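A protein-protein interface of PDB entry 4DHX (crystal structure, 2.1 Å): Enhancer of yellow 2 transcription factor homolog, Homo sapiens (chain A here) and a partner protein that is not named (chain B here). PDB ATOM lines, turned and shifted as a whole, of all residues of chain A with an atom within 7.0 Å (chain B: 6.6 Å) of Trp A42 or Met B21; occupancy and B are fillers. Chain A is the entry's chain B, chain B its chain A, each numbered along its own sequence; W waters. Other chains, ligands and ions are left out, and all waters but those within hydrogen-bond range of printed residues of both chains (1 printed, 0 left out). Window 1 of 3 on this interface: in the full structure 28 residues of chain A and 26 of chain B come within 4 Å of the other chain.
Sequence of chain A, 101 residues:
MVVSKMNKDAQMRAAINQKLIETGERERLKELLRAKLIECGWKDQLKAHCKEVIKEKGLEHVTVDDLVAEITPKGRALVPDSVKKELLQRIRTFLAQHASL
Trp A42 touches three residues of chain B. Of the printed residues of chain A, Met B21 touches Trp A42 and Arg A76. Of the printed residues of chain B, Arg A76 touches Glu B18, Met B21 and Met B22. Printed residues of chain A within 4 Å of Met B22: Thr A72 (3.6 Å) and Arg A76 (3.8 Å). Of the printed residues of chain A, Glu B18 touches Arg A76 (3.0 Å). Of the printed residues of chain A, Thr B28 touches Lys A43 and Lys A47. Printed residues of chain A within 4 Å of Val B20: Arg A34. The nearest printed residue of chain A that does not touch Met B21 is Val A79 (4.01 Å). The nearest printed residue of chain B that does not touch Val A79 is Met B21 (4.01 Å).
The backbone carbonyl oxygen of Leu A37 lies within hydrogen-bond range of the backbone NH of Trp A42 (3.0 Å). The backbone carbonyl oxygen (O) of Phe B24 lies within hydrogen-bond range of the side-chain hydroxyl (OG1) of Thr B28 (2.8 Å). The side-chain carboxylate (OD1) of Asp A44 is in salt-bridge range of the side-chain amino group (NZ) of Lys A47 (3.9 Å). NE1 of Trp A42 is in hydrogen-bond range of O of Gly A75 (2.9 Å). The side-chain sulfur (SG) of Cys A40 sits close to the backbone NH (N) of Trp A42 (3.7 Å).
Hydrophobic or aromatic side chains of chain A within 4 Å of the printed part of chain B: Leu A33, Ile A38, Trp A42, Leu A46 and Val A79. Among the printed residues, 17 pairs touch across the chains.
The guanidinium group of Arg A76 lies within salt-bridge range of the side-chain carboxylate of Glu B18 (3.0 Å).
CE of Met B17 touches CD2 of Leu A33 (3.6 Å). Phe B24 touches Ile A38. CZ3 of Trp A42 touches CD2 of Phe B24, 3.9 Å away. Trp A42 touches Val B25 (CH2 to CG2, 3.98 Å). Thr B28 touches Lys A43 (OG1 to CE, 3.8 Å). CG of Lys A47 touches CG2 of Thr B28 (3.7 Å). Thr A72 touches Met B22 (CG2 to CE, 3.6 Å). OG1 of Thr A72 touches CG1 of Val B25, 3.7 Å away. Arg A76 touches Met B21. Val A79 touches Met B17.
Water W1 lies within hydrogen-bond range of the side-chain carboxylate of Glu B23 (2.7 Å), the backbone carbonyl oxygen of Val B20 (2.9 Å) and the guanidinium group of Arg A34 (3.0 Å).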
ATOM      1  N   LEU A  33      23.043 -25.434 -23.587  1.00  0.00           N
ATOM      2  CA  LEU A  33      23.221 -24.382 -24.584  1.00  0.00           C
ATOM      3  C   LEU A  33      24.441 -23.534 -24.245  1.00  0.00           C
ATOM      4  O   LEU A  33      25.306 -23.305 -25.088  1.00  0.00           O
ATOM      5  CB  LEU A  33      21.981 -23.490 -24.658  1.00  0.00           C
ATOM      6  CG  LEU A  33      20.823 -23.982 -25.528  1.00  0.00           C
ATOM      7  CD1 LEU A  33      19.601 -23.103 -25.324  1.00  0.00           C
ATOM      8  CD2 LEU A  33      21.226 -24.000 -26.996  1.00  0.00           C
ATOM      9  N   ARG A  34      24.499 -23.067 -23.002  1.00  0.00           N
ATOM     10  CA  ARG A  34      25.608 -22.240 -22.543  1.00  0.00           C
ATOM     11  C   ARG A  34      26.934 -22.982 -22.685  1.00  0.00           C
ATOM     12  O   ARG A  34      27.942 -22.402 -23.097  1.00  0.00           O
ATOM     13  CB  ARG A  34      25.385 -21.821 -21.088  1.00  0.00           C
ATOM     14  CG  ARG A  34      24.267 -20.799 -20.915  1.00  0.00           C
ATOM     15  CD  ARG A  34      23.873 -20.617 -19.454  1.00  0.00           C
ATOM     16  NE  ARG A  34      24.993 -20.184 -18.621  1.00  0.00           N
ATOM     17  CZ  ARG A  34      25.379 -18.920 -18.462  1.00  0.00           C
ATOM     18  NH1 ARG A  34      24.748 -17.930 -19.084  1.00  0.00           N
ATOM     19  NH2 ARG A  34      26.408 -18.641 -17.677  1.00  0.00           N
ATOM     20  N   LYS A  36      27.658 -25.406 -24.796  1.00  0.00           N
ATOM     21  CA  LYS A  36      28.002 -25.581 -26.205  1.00  0.00           C
ATOM     22  C   LYS A  36      28.544 -24.281 -26.794  1.00  0.00           C
ATOM     23  O   LYS A  36      29.469 -24.295 -27.607  1.00  0.00           O
ATOM     24  CB  LYS A  36      26.783 -26.047 -27.008  1.00  0.00           C
ATOM     25  CG  LYS A  36      27.094 -27.123 -28.041  1.00  0.00           C
ATOM     26  CD  LYS A  36      27.437 -28.448 -27.369  1.00  0.00           C
ATOM     27  CE  LYS A  36      27.760 -29.540 -28.375  1.00  0.00           C
ATOM     28  NZ  LYS A  36      28.156 -30.804 -27.693  1.00  0.00           N
ATOM     29  N   LEU A  37      27.964 -23.158 -26.381  1.00  0.00           N
ATOM     30  CA  LEU A  37      28.413 -21.851 -26.851  1.00  0.00           C
ATOM     31  C   LEU A  37      29.821 -21.547 -26.346  1.00  0.00           C
ATOM     32  O   LEU A  37      30.627 -20.933 -27.048  1.00  0.00           O
ATOM     33  CB  LEU A  37      27.441 -20.758 -26.401  1.00  0.00           C
ATOM     34  CG  LEU A  37      26.116 -20.703 -27.168  1.00  0.00           C
ATOM     35  CD1 LEU A  37      25.175 -19.683 -26.546  1.00  0.00           C
ATOM     36  CD2 LEU A  37      26.355 -20.381 -28.637  1.00  0.00           C
ATOM     37  N   ILE A  38      30.112 -21.983 -25.126  1.00  0.00           N
ATOM     38  CA  ILE A  38      31.447 -21.834 -24.568  1.00  0.00           C
ATOM     39  C   ILE A  38      32.428 -22.730 -25.313  1.00  0.00           C
ATOM     40  O   ILE A  38      33.540 -22.314 -25.645  1.00  0.00           O
ATOM     41  CB  ILE A  38      31.470 -22.196 -23.075  1.00  0.00           C
ATOM     42  CG1 ILE A  38      30.760 -21.111 -22.264  1.00  0.00           C
ATOM     43  CG2 ILE A  38      32.904 -22.359 -22.585  1.00  0.00           C
ATOM     44  CD1 ILE A  38      30.586 -21.457 -20.802  1.00  0.00           C
ATOM     45  N   GLU A  39      32.005 -23.960 -25.580  1.00  0.00           N
ATOM     46  CA  GLU A  39      32.866 -24.951 -26.211  1.00  0.00           C
ATOM     47  C   GLU A  39      33.303 -24.542 -27.617  1.00  0.00           C
ATOM     48  O   GLU A  39      34.456 -24.745 -27.997  1.00  0.00           O
ATOM     49  CB  GLU A  39      32.160 -26.308 -26.268  1.00  0.00           C
ATOM     50  CG  GLU A  39      33.042 -27.438 -26.777  1.00  0.00           C
ATOM     51  CD  GLU A  39      32.313 -28.766 -26.859  1.00  0.00           C
ATOM     52  OE1 GLU A  39      31.066 -28.769 -26.819  1.00  0.00           O
ATOM     53  OE2 GLU A  39      32.992 -29.811 -26.963  1.00  0.00           O
ATOM     54  N   CYS A  40      32.384 -23.970 -28.391  1.00  0.00           N
ATOM     55  CA  CYS A  40      32.668 -23.644 -29.787  1.00  0.00           C
ATOM     56  C   CYS A  40      33.408 -22.313 -29.947  1.00  0.00           C
ATOM     57  O   CYS A  40      33.758 -21.927 -31.061  1.00  0.00           O
ATOM     58  CB  CYS A  40      31.376 -23.626 -30.609  1.00  0.00           C
ATOM     59  SG  CYS A  40      30.297 -22.215 -30.291  1.00  0.00           S
ATOM     60  N   GLY A  41      33.642 -21.617 -28.839  1.00  0.00           N
ATOM     61  CA  GLY A  41      34.406 -20.382 -28.866  1.00  0.00           C
ATOM     62  C   GLY A  41      33.550 -19.139 -29.032  1.00  0.00           C
ATOM     63  O   GLY A  41      34.074 -18.032 -29.162  1.00  0.00           O
ATOM     64  N   TRP A  42      32.233 -19.320 -29.025  1.00  0.00           N
ATOM     65  CA  TRP A  42      31.298 -18.212 -29.199  1.00  0.00           C
ATOM     66  C   TRP A  42      31.473 -17.151 -28.111  1.00  0.00           C
ATOM     67  O   TRP A  42      31.404 -15.953 -28.387  1.00  0.00           O
ATOM     68  CB  TRP A  42      29.859 -18.735 -29.195  1.00  0.00           C
ATOM     69  CG  TRP A  42      28.815 -17.679 -29.415  1.00  0.00           C
ATOM     70  CD1 TRP A  42      28.387 -17.185 -30.613  1.00  0.00           C
ATOM     71  CD2 TRP A  42      28.057 -16.997 -28.409  1.00  0.00           C
ATOM     72  NE1 TRP A  42      27.414 -16.236 -30.415  1.00  0.00           N
ATOM     73  CE2 TRP A  42      27.193 -16.102 -29.070  1.00  0.00           C
ATOM     74  CE3 TRP A  42      28.026 -17.058 -27.012  1.00  0.00           C
ATOM     75  CZ2 TRP A  42      26.309 -15.273 -28.384  1.00  0.00           C
ATOM     76  CZ3 TRP A  42      27.147 -16.233 -26.332  1.00  0.00           C
ATOM     77  CH2 TRP A  42      26.300 -15.354 -27.018  1.00  0.00           C
ATOM     78  N   LYS A  43      31.699 -17.588 -26.876  1.00  0.00           N
ATOM     79  CA  LYS A  43      31.843 -16.651 -25.767  1.00  0.00           C
ATOM     80  C   LYS A  43      33.163 -15.887 -25.851  1.00  0.00           C
ATOM     81  O   LYS A  43      33.235 -14.716 -25.480  1.00  0.00           O
ATOM     82  CB  LYS A  43      31.747 -17.367 -24.419  1.00  0.00           C
ATOM     83  CG  LYS A  43      31.798 -16.406 -23.238  1.00  0.00           C
ATOM     84  CD  LYS A  43      31.876 -17.124 -21.905  1.00  0.00           C
ATOM     85  CE  LYS A  43      32.009 -16.126 -20.766  1.00  0.00           C
ATOM     86  NZ  LYS A  43      32.084 -16.796 -19.441  1.00  0.00           N
ATOM     87  N   ASP A  44      34.209 -16.554 -26.330  1.00  0.00           N
ATOM     88  CA  ASP A  44      35.501 -15.905 -26.518  1.00  0.00           C
ATOM     89  C   ASP A  44      35.388 -14.797 -27.562  1.00  0.00           C
ATOM     90  O   ASP A  44      36.069 -13.776 -27.471  1.00  0.00           O
ATOM     91  CB  ASP A  44      36.568 -16.918 -26.943  1.00  0.00           C
ATOM     92  CG  ASP A  44      36.993 -17.832 -25.808  1.00  0.00           C
ATOM     93  OD1 ASP A  44      36.839 -17.438 -24.633  1.00  0.00           O
ATOM     94  OD2 ASP A  44      37.490 -18.943 -26.094  1.00  0.00           O
ATOM     95  N   GLN A  45      34.525 -15.006 -28.554  1.00  0.00           N
ATOM     96  CA  GLN A  45      34.286 -14.001 -29.584  1.00  0.00           C
ATOM     97  C   GLN A  45      33.625 -12.764 -28.985  1.00  0.00           C
ATOM     98  O   GLN A  45      33.954 -11.641 -29.359  1.00  0.00           O
ATOM     99  CB  GLN A  45      33.415 -14.570 -30.708  1.00  0.00           C
ATOM    100  CG  GLN A  45      34.143 -15.542 -31.624  1.00  0.00           C
ATOM    101  CD  GLN A  45      33.213 -16.216 -32.620  1.00  0.00           C
ATOM    102  OE1 GLN A  45      32.016 -16.363 -32.371  1.00  0.00           O
ATOM    103  NE2 GLN A  45      33.763 -16.630 -33.756  1.00  0.00           N
ATOM    104  N   LEU A  46      32.694 -12.971 -28.058  1.00  0.00           N
ATOM    105  CA  LEU A  46      32.047 -11.857 -27.371  1.00  0.00           C
ATOM    106  C   LEU A  46      33.076 -11.036 -26.604  1.00  0.00           C
ATOM    107  O   LEU A  46      33.076  -9.806 -26.659  1.00  0.00           O
ATOM    108  CB  LEU A  46      30.985 -12.356 -26.391  1.00  0.00           C
ATOM    109  CG  LEU A  46      29.683 -12.928 -26.950  1.00  0.00           C
ATOM    110  CD1 LEU A  46      28.747 -13.249 -25.797  1.00  0.00           C
ATOM    111  CD2 LEU A  46      29.027 -11.963 -27.927  1.00  0.00           C
ATOM    112  N   LYS A  47      33.951 -11.728 -25.882  1.00  0.00           N
ATOM    113  CA  LYS A  47      34.951 -11.067 -25.054  1.00  0.00           C
ATOM    114  C   LYS A  47      35.936 -10.282 -25.910  1.00  0.00           C
ATOM    115  O   LYS A  47      36.311  -9.163 -25.567  1.00  0.00           O
ATOM    116  CB  LYS A  47      35.691 -12.091 -24.192  1.00  0.00           C
ATOM    117  CG  LYS A  47      34.830 -12.676 -23.086  1.00  0.00           C
ATOM    118  CD  LYS A  47      35.658 -13.384 -22.023  1.00  0.00           C
ATOM    119  CE  LYS A  47      35.967 -14.819 -22.403  1.00  0.00           C
ATOM    120  NZ  LYS A  47      36.181 -15.663 -21.192  1.00  0.00           N
ATOM    121  N   THR A  72      25.753  -7.176 -29.305  1.00  0.00           N
ATOM    122  CA  THR A  72      24.655  -8.128 -29.467  1.00  0.00           C
ATOM    123  C   THR A  72      24.439  -8.585 -30.912  1.00  0.00           C
ATOM    124  O   THR A  72      24.447  -9.785 -31.183  1.00  0.00           O
ATOM    125  CB  THR A  72      23.337  -7.572 -28.891  1.00  0.00           C
ATOM    126  OG1 THR A  72      23.371  -7.654 -27.461  1.00  0.00           O
ATOM    127  CG2 THR A  72      22.147  -8.367 -29.405  1.00  0.00           C
ATOM    128  N   PRO A  73      24.240  -7.636 -31.843  1.00  0.00           N
ATOM    129  CA  PRO A  73      23.966  -8.006 -33.238  1.00  0.00           C
ATOM    130  C   PRO A  73      24.904  -9.083 -33.785  1.00  0.00           C
ATOM    131  O   PRO A  73      24.436 -10.074 -34.343  1.00  0.00           O
ATOM    132  CB  PRO A  73      24.173  -6.689 -33.989  1.00  0.00           C
ATOM    133  CG  PRO A  73      23.809  -5.648 -33.001  1.00  0.00           C
ATOM    134  CD  PRO A  73      24.246  -6.173 -31.658  1.00  0.00           C
ATOM    135  N   LYS A  74      26.209  -8.884 -33.628  1.00  0.00           N
ATOM    136  CA  LYS A  74      27.189  -9.852 -34.107  1.00  0.00           C
ATOM    137  C   LYS A  74      27.082 -11.156 -33.321  1.00  0.00           C
ATOM    138  O   LYS A  74      27.198 -12.242 -33.889  1.00  0.00           O
ATOM    139  CB  LYS A  74      28.602  -9.276 -34.003  1.00  0.00           C
ATOM    140  CG  LYS A  74      29.704 -10.232 -34.437  1.00  0.00           C
ATOM    141  CD  LYS A  74      30.978  -9.475 -34.784  1.00  0.00           C
ATOM    142  CE  LYS A  74      32.155 -10.414 -34.998  1.00  0.00           C
ATOM    143  NZ  LYS A  74      32.699 -10.938 -33.712  1.00  0.00           N
ATOM    144  N   GLY A  75      26.854 -11.047 -32.016  1.00  0.00           N
ATOM    145  CA  GLY A  75      26.679 -12.220 -31.178  1.00  0.00           C
ATOM    146  C   GLY A  75      25.540 -13.093 -31.672  1.00  0.00           C
ATOM    147  O   GLY A  75      25.691 -14.304 -31.826  1.00  0.00           O
ATOM    148  N   ARG A  76      24.395 -12.471 -31.926  1.00  0.00           N
ATOM    149  CA  ARG A  76      23.225 -13.181 -32.415  1.00  0.00           C
ATOM    150  C   ARG A  76      23.514 -13.880 -33.736  1.00  0.00           C
ATOM    151  O   ARG A  76      23.040 -14.990 -33.976  1.00  0.00           O
ATOM    152  CB  ARG A  76      22.055 -12.211 -32.595  1.00  0.00           C
ATOM    153  CG  ARG A  76      20.788 -12.872 -33.115  1.00  0.00           C
ATOM    154  CD  ARG A  76      19.633 -11.890 -33.247  1.00  0.00           C
ATOM    155  NE  ARG A  76      19.279 -11.268 -31.970  1.00  0.00           N
ATOM    156  CZ  ARG A  76      19.506  -9.997 -31.642  1.00  0.00           C
ATOM    157  NH1 ARG A  76      20.091  -9.157 -32.488  1.00  0.00           N
ATOM    158  NH2 ARG A  76      19.139  -9.552 -30.450  1.00  0.00           N
ATOM    159  N   ALA A  77      24.291 -13.226 -34.591  1.00  0.00           N
ATOM    160  CA  ALA A  77      24.561 -13.747 -35.923  1.00  0.00           C
ATOM    161  C   ALA A  77      25.586 -14.880 -35.922  1.00  0.00           C
ATOM    162  O   ALA A  77      25.688 -15.623 -36.897  1.00  0.00           O
ATOM    163  CB  ALA A  77      25.024 -12.623 -36.835  1.00  0.00           C
ATOM    164  N   LEU A  78      26.340 -15.017 -34.835  1.00  0.00           N
ATOM    165  CA  LEU A  78      27.402 -16.021 -34.773  1.00  0.00           C
ATOM    166  C   LEU A  78      26.985 -17.295 -34.039  1.00  0.00           C
ATOM    167  O   LEU A  78      27.759 -18.248 -33.961  1.00  0.00           O
ATOM    168  CB  LEU A  78      28.657 -15.431 -34.125  1.00  0.00           C
ATOM    169  CG  LEU A  78      29.362 -14.329 -34.920  1.00  0.00           C
ATOM    170  CD1 LEU A  78      30.638 -13.899 -34.215  1.00  0.00           C
ATOM    171  CD2 LEU A  78      29.663 -14.778 -36.342  1.00  0.00           C
ATOM    172  N   VAL A  79      25.771 -17.317 -33.497  1.00  0.00           N
ATOM    173  CA  VAL A  79      25.243 -18.547 -32.916  1.00  0.00           C
ATOM    174  C   VAL A  79      25.148 -19.591 -34.026  1.00  0.00           C
ATOM    175  O   VAL A  79      24.415 -19.396 -34.992  1.00  0.00           O
ATOM    176  CB  VAL A  79      23.849 -18.343 -32.287  1.00  0.00           C
ATOM    177  CG1 VAL A  79      23.292 -19.669 -31.785  1.00  0.00           C
ATOM    178  CG2 VAL A  79      23.920 -17.331 -31.152  1.00  0.00           C
ATOM    179  N   PRO A  80      25.899 -20.697 -33.900  1.00  0.00           N
ATOM    180  CA  PRO A  80      25.926 -21.702 -34.971  1.00  0.00           C
ATOM    181  C   PRO A  80      24.547 -22.285 -35.256  1.00  0.00           C
ATOM    182  O   PRO A  80      23.777 -22.521 -34.327  1.00  0.00           O
ATOM    183  CB  PRO A  80      26.854 -22.791 -34.414  1.00  0.00           C
ATOM    184  CG  PRO A  80      27.624 -22.136 -33.317  1.00  0.00           C
ATOM    185  CD  PRO A  80      26.722 -21.097 -32.746  1.00  0.00           C
ATOM    186  N   LEU B  16      13.685 -19.360 -26.836  1.00  0.00           N
ATOM    187  CA  LEU B  16      14.564 -19.913 -25.814  1.00  0.00           C
ATOM    188  C   LEU B  16      16.019 -19.592 -26.135  1.00  0.00           C
ATOM    189  O   LEU B  16      16.775 -19.164 -25.264  1.00  0.00           O
ATOM    190  CB  LEU B  16      14.371 -21.426 -25.709  1.00  0.00           C
ATOM    191  CG  LEU B  16      15.366 -22.168 -24.813  1.00  0.00           C
ATOM    192  CD1 LEU B  16      15.428 -21.539 -23.429  1.00  0.00           C
ATOM    193  CD2 LEU B  16      14.996 -23.640 -24.711  1.00  0.00           C
ATOM    194  N   MET B  17      16.400 -19.801 -27.390  1.00  0.00           N
ATOM    195  CA  MET B  17      17.755 -19.516 -27.839  1.00  0.00           C
ATOM    196  C   MET B  17      18.078 -18.035 -27.665  1.00  0.00           C
ATOM    197  O   MET B  17      19.170 -17.680 -27.219  1.00  0.00           O
ATOM    198  CB  MET B  17      17.924 -19.925 -29.305  1.00  0.00           C
ATOM    199  CG  MET B  17      19.291 -19.603 -29.888  1.00  0.00           C
ATOM    200  SD  MET B  17      20.640 -20.422 -29.013  1.00  0.00           S
ATOM    201  CE  MET B  17      20.745 -21.972 -29.890  1.00  0.00           C
ATOM    202  N   GLU B  18      17.121 -17.177 -28.008  1.00  0.00           N
ATOM    203  CA  GLU B  18      17.313 -15.732 -27.933  1.00  0.00           C
ATOM    204  C   GLU B  18      17.456 -15.243 -26.490  1.00  0.00           C
ATOM    205  O   GLU B  18      18.275 -14.369 -26.204  1.00  0.00           O
ATOM    206  CB  GLU B  18      16.150 -15.011 -28.625  1.00  0.00           C
ATOM    207  CG  GLU B  18      16.185 -13.493 -28.509  1.00  0.00           C
ATOM    208  CD  GLU B  18      17.342 -12.867 -29.271  1.00  0.00           C
ATOM    209  OE1 GLU B  18      17.930 -13.550 -30.137  1.00  0.00           O
ATOM    210  OE2 GLU B  18      17.662 -11.689 -29.005  1.00  0.00           O
ATOM    211  N   ARG B  19      16.664 -15.806 -25.582  1.00  0.00           N
ATOM    212  CA  ARG B  19      16.722 -15.410 -24.177  1.00  0.00           C
ATOM    213  C   ARG B  19      18.027 -15.856 -23.522  1.00  0.00           C
ATOM    214  O   ARG B  19      18.656 -15.091 -22.793  1.00  0.00           O
ATOM    215  CB  ARG B  19      15.533 -15.979 -23.402  1.00  0.00           C
ATOM    216  CG  ARG B  19      14.235 -15.220 -23.611  1.00  0.00           C
ATOM    217  CD  ARG B  19      13.100 -15.821 -22.797  1.00  0.00           C
ATOM    218  NE  ARG B  19      11.862 -15.059 -22.941  1.00  0.00           N
ATOM    219  CZ  ARG B  19      11.512 -14.027 -22.177  1.00  0.00           C
ATOM    220  NH1 ARG B  19      12.298 -13.609 -21.193  1.00  0.00           N
ATOM    221  NH2 ARG B  19      10.363 -13.405 -22.398  1.00  0.00           N
ATOM    222  N   VAL B  20      18.425 -17.099 -23.773  1.00  0.00           N
ATOM    223  CA  VAL B  20      19.675 -17.616 -23.228  1.00  0.00           C
ATOM    224  C   VAL B  20      20.863 -16.836 -23.786  1.00  0.00           C
ATOM    225  O   VAL B  20      21.785 -16.480 -23.053  1.00  0.00           O
ATOM    226  CB  VAL B  20      19.850 -19.117 -23.535  1.00  0.00           C
ATOM    227  CG1 VAL B  20      21.247 -19.587 -23.146  1.00  0.00           C
ATOM    228  CG2 VAL B  20      18.796 -19.927 -22.802  1.00  0.00           C
ATOM    229  N   MET B  21      20.827 -16.569 -25.087  1.00  0.00           N
ATOM    230  CA  MET B  21      21.893 -15.844 -25.764  1.00  0.00           C
ATOM    231  C   MET B  21      22.023 -14.430 -25.207  1.00  0.00           C
ATOM    232  O   MET B  21      23.122 -13.981 -24.876  1.00  0.00           O
ATOM    233  CB  MET B  21      21.597 -15.797 -27.263  1.00  0.00           C
ATOM    234  CG  MET B  21      22.638 -15.072 -28.094  1.00  0.00           C
ATOM    235  SD  MET B  21      22.312 -13.307 -28.256  1.00  0.00           S
ATOM    236  CE  MET B  21      20.875 -13.291 -29.327  1.00  0.00           C
ATOM    237  N   MET B  22      20.895 -13.736 -25.097  1.00  0.00           N
ATOM    238  CA  MET B  22      20.881 -12.366 -24.599  1.00  0.00           C
ATOM    239  C   MET B  22      21.454 -12.278 -23.187  1.00  0.00           C
ATOM    240  O   MET B  22      22.308 -11.437 -22.914  1.00  0.00           O
ATOM    241  CB  MET B  22      19.458 -11.810 -24.616  1.00  0.00           C
ATOM    242  CG  MET B  22      19.357 -10.346 -24.233  1.00  0.00           C
ATOM    243  SD  MET B  22      20.470  -9.294 -25.189  1.00  0.00           S
ATOM    244  CE  MET B  22      20.171  -9.912 -26.841  1.00  0.00           C
ATOM    245  N   GLU B  23      20.980 -13.140 -22.290  1.00  0.00           N
ATOM    246  CA  GLU B  23      21.466 -13.140 -20.913  1.00  0.00           C
ATOM    247  C   GLU B  23      22.967 -13.397 -20.862  1.00  0.00           C
ATOM    248  O   GLU B  23      23.666 -12.861 -20.003  1.00  0.00           O
ATOM    249  CB  GLU B  23      20.747 -14.195 -20.069  1.00  0.00           C
ATOM    250  CG  GLU B  23      21.229 -14.235 -18.622  1.00  0.00           C
ATOM    251  CD  GLU B  23      20.603 -15.355 -17.815  1.00  0.00           C
ATOM    252  OE1 GLU B  23      20.026 -15.065 -16.745  1.00  0.00           O
ATOM    253  OE2 GLU B  23      20.699 -16.526 -18.240  1.00  0.00           O
ATOM    254  N   PHE B  24      23.459 -14.224 -21.778  1.00  0.00           N
ATOM    255  CA  PHE B  24      24.878 -14.561 -21.804  1.00  0.00           C
ATOM    256  C   PHE B  24      25.694 -13.346 -22.242  1.00  0.00           C
ATOM    257  O   PHE B  24      26.785 -13.103 -21.727  1.00  0.00           O
ATOM    258  CB  PHE B  24      25.135 -15.742 -22.745  1.00  0.00           C
ATOM    259  CG  PHE B  24      26.259 -16.648 -22.302  1.00  0.00           C
ATOM    260  CD1 PHE B  24      27.127 -16.270 -21.289  1.00  0.00           C
ATOM    261  CD2 PHE B  24      26.442 -17.884 -22.903  1.00  0.00           C
ATOM    262  CE1 PHE B  24      28.151 -17.105 -20.888  1.00  0.00           C
ATOM    263  CE2 PHE B  24      27.465 -18.721 -22.504  1.00  0.00           C
ATOM    264  CZ  PHE B  24      28.320 -18.331 -21.496  1.00  0.00           C
ATOM    265  N   VAL B  25      25.159 -12.581 -23.189  1.00  0.00           N
ATOM    266  CA  VAL B  25      25.826 -11.368 -23.649  1.00  0.00           C
ATOM    267  C   VAL B  25      25.908 -10.346 -22.517  1.00  0.00           C
ATOM    268  O   VAL B  25      26.951  -9.730 -22.298  1.00  0.00           O
ATOM    269  CB  VAL B  25      25.101 -10.736 -24.857  1.00  0.00           C
ATOM    270  CG1 VAL B  25      25.698  -9.373 -25.187  1.00  0.00           C
ATOM    271  CG2 VAL B  25      25.178 -11.655 -26.071  1.00  0.00           C
ATOM    272  N   ARG B  26      24.804 -10.175 -21.796  1.00  0.00           N
ATOM    273  CA  ARG B  26      24.752  -9.213 -20.699  1.00  0.00           C
ATOM    274  C   ARG B  26      25.749  -9.569 -19.602  1.00  0.00           C
ATOM    275  O   ARG B  26      26.477  -8.704 -19.110  1.00  0.00           O
ATOM    276  CB  ARG B  26      23.341  -9.132 -20.115  1.00  0.00           C
ATOM    277  CG  ARG B  26      22.292  -8.610 -21.089  1.00  0.00           C
ATOM    278  CD  ARG B  26      20.935  -8.480 -20.422  1.00  0.00           C
ATOM    279  NE  ARG B  26      20.937  -7.440 -19.395  1.00  0.00           N
ATOM    280  CZ  ARG B  26      20.397  -7.558 -18.184  1.00  0.00           C
ATOM    281  NH1 ARG B  26      19.785  -8.674 -17.811  1.00  0.00           N
ATOM    282  NH2 ARG B  26      20.466  -6.545 -17.334  1.00  0.00           N
ATOM    283  N   THR B  28      28.414 -11.429 -19.905  1.00  0.00           N
ATOM    284  CA  THR B  28      29.770 -11.354 -20.434  1.00  0.00           C
ATOM    285  C   THR B  28      30.262  -9.908 -20.465  1.00  0.00           C
ATOM    286  O   THR B  28      31.377  -9.617 -20.035  1.00  0.00           O
ATOM    287  CB  THR B  28      29.864 -11.960 -21.847  1.00  0.00           C
ATOM    288  OG1 THR B  28      29.550 -13.356 -21.792  1.00  0.00           O
ATOM    289  CG2 THR B  28      31.267 -11.786 -22.418  1.00  0.00           C
HETATM  290  O   HOH W   1      22.083 -17.508 -20.324  1.00  0.00           O
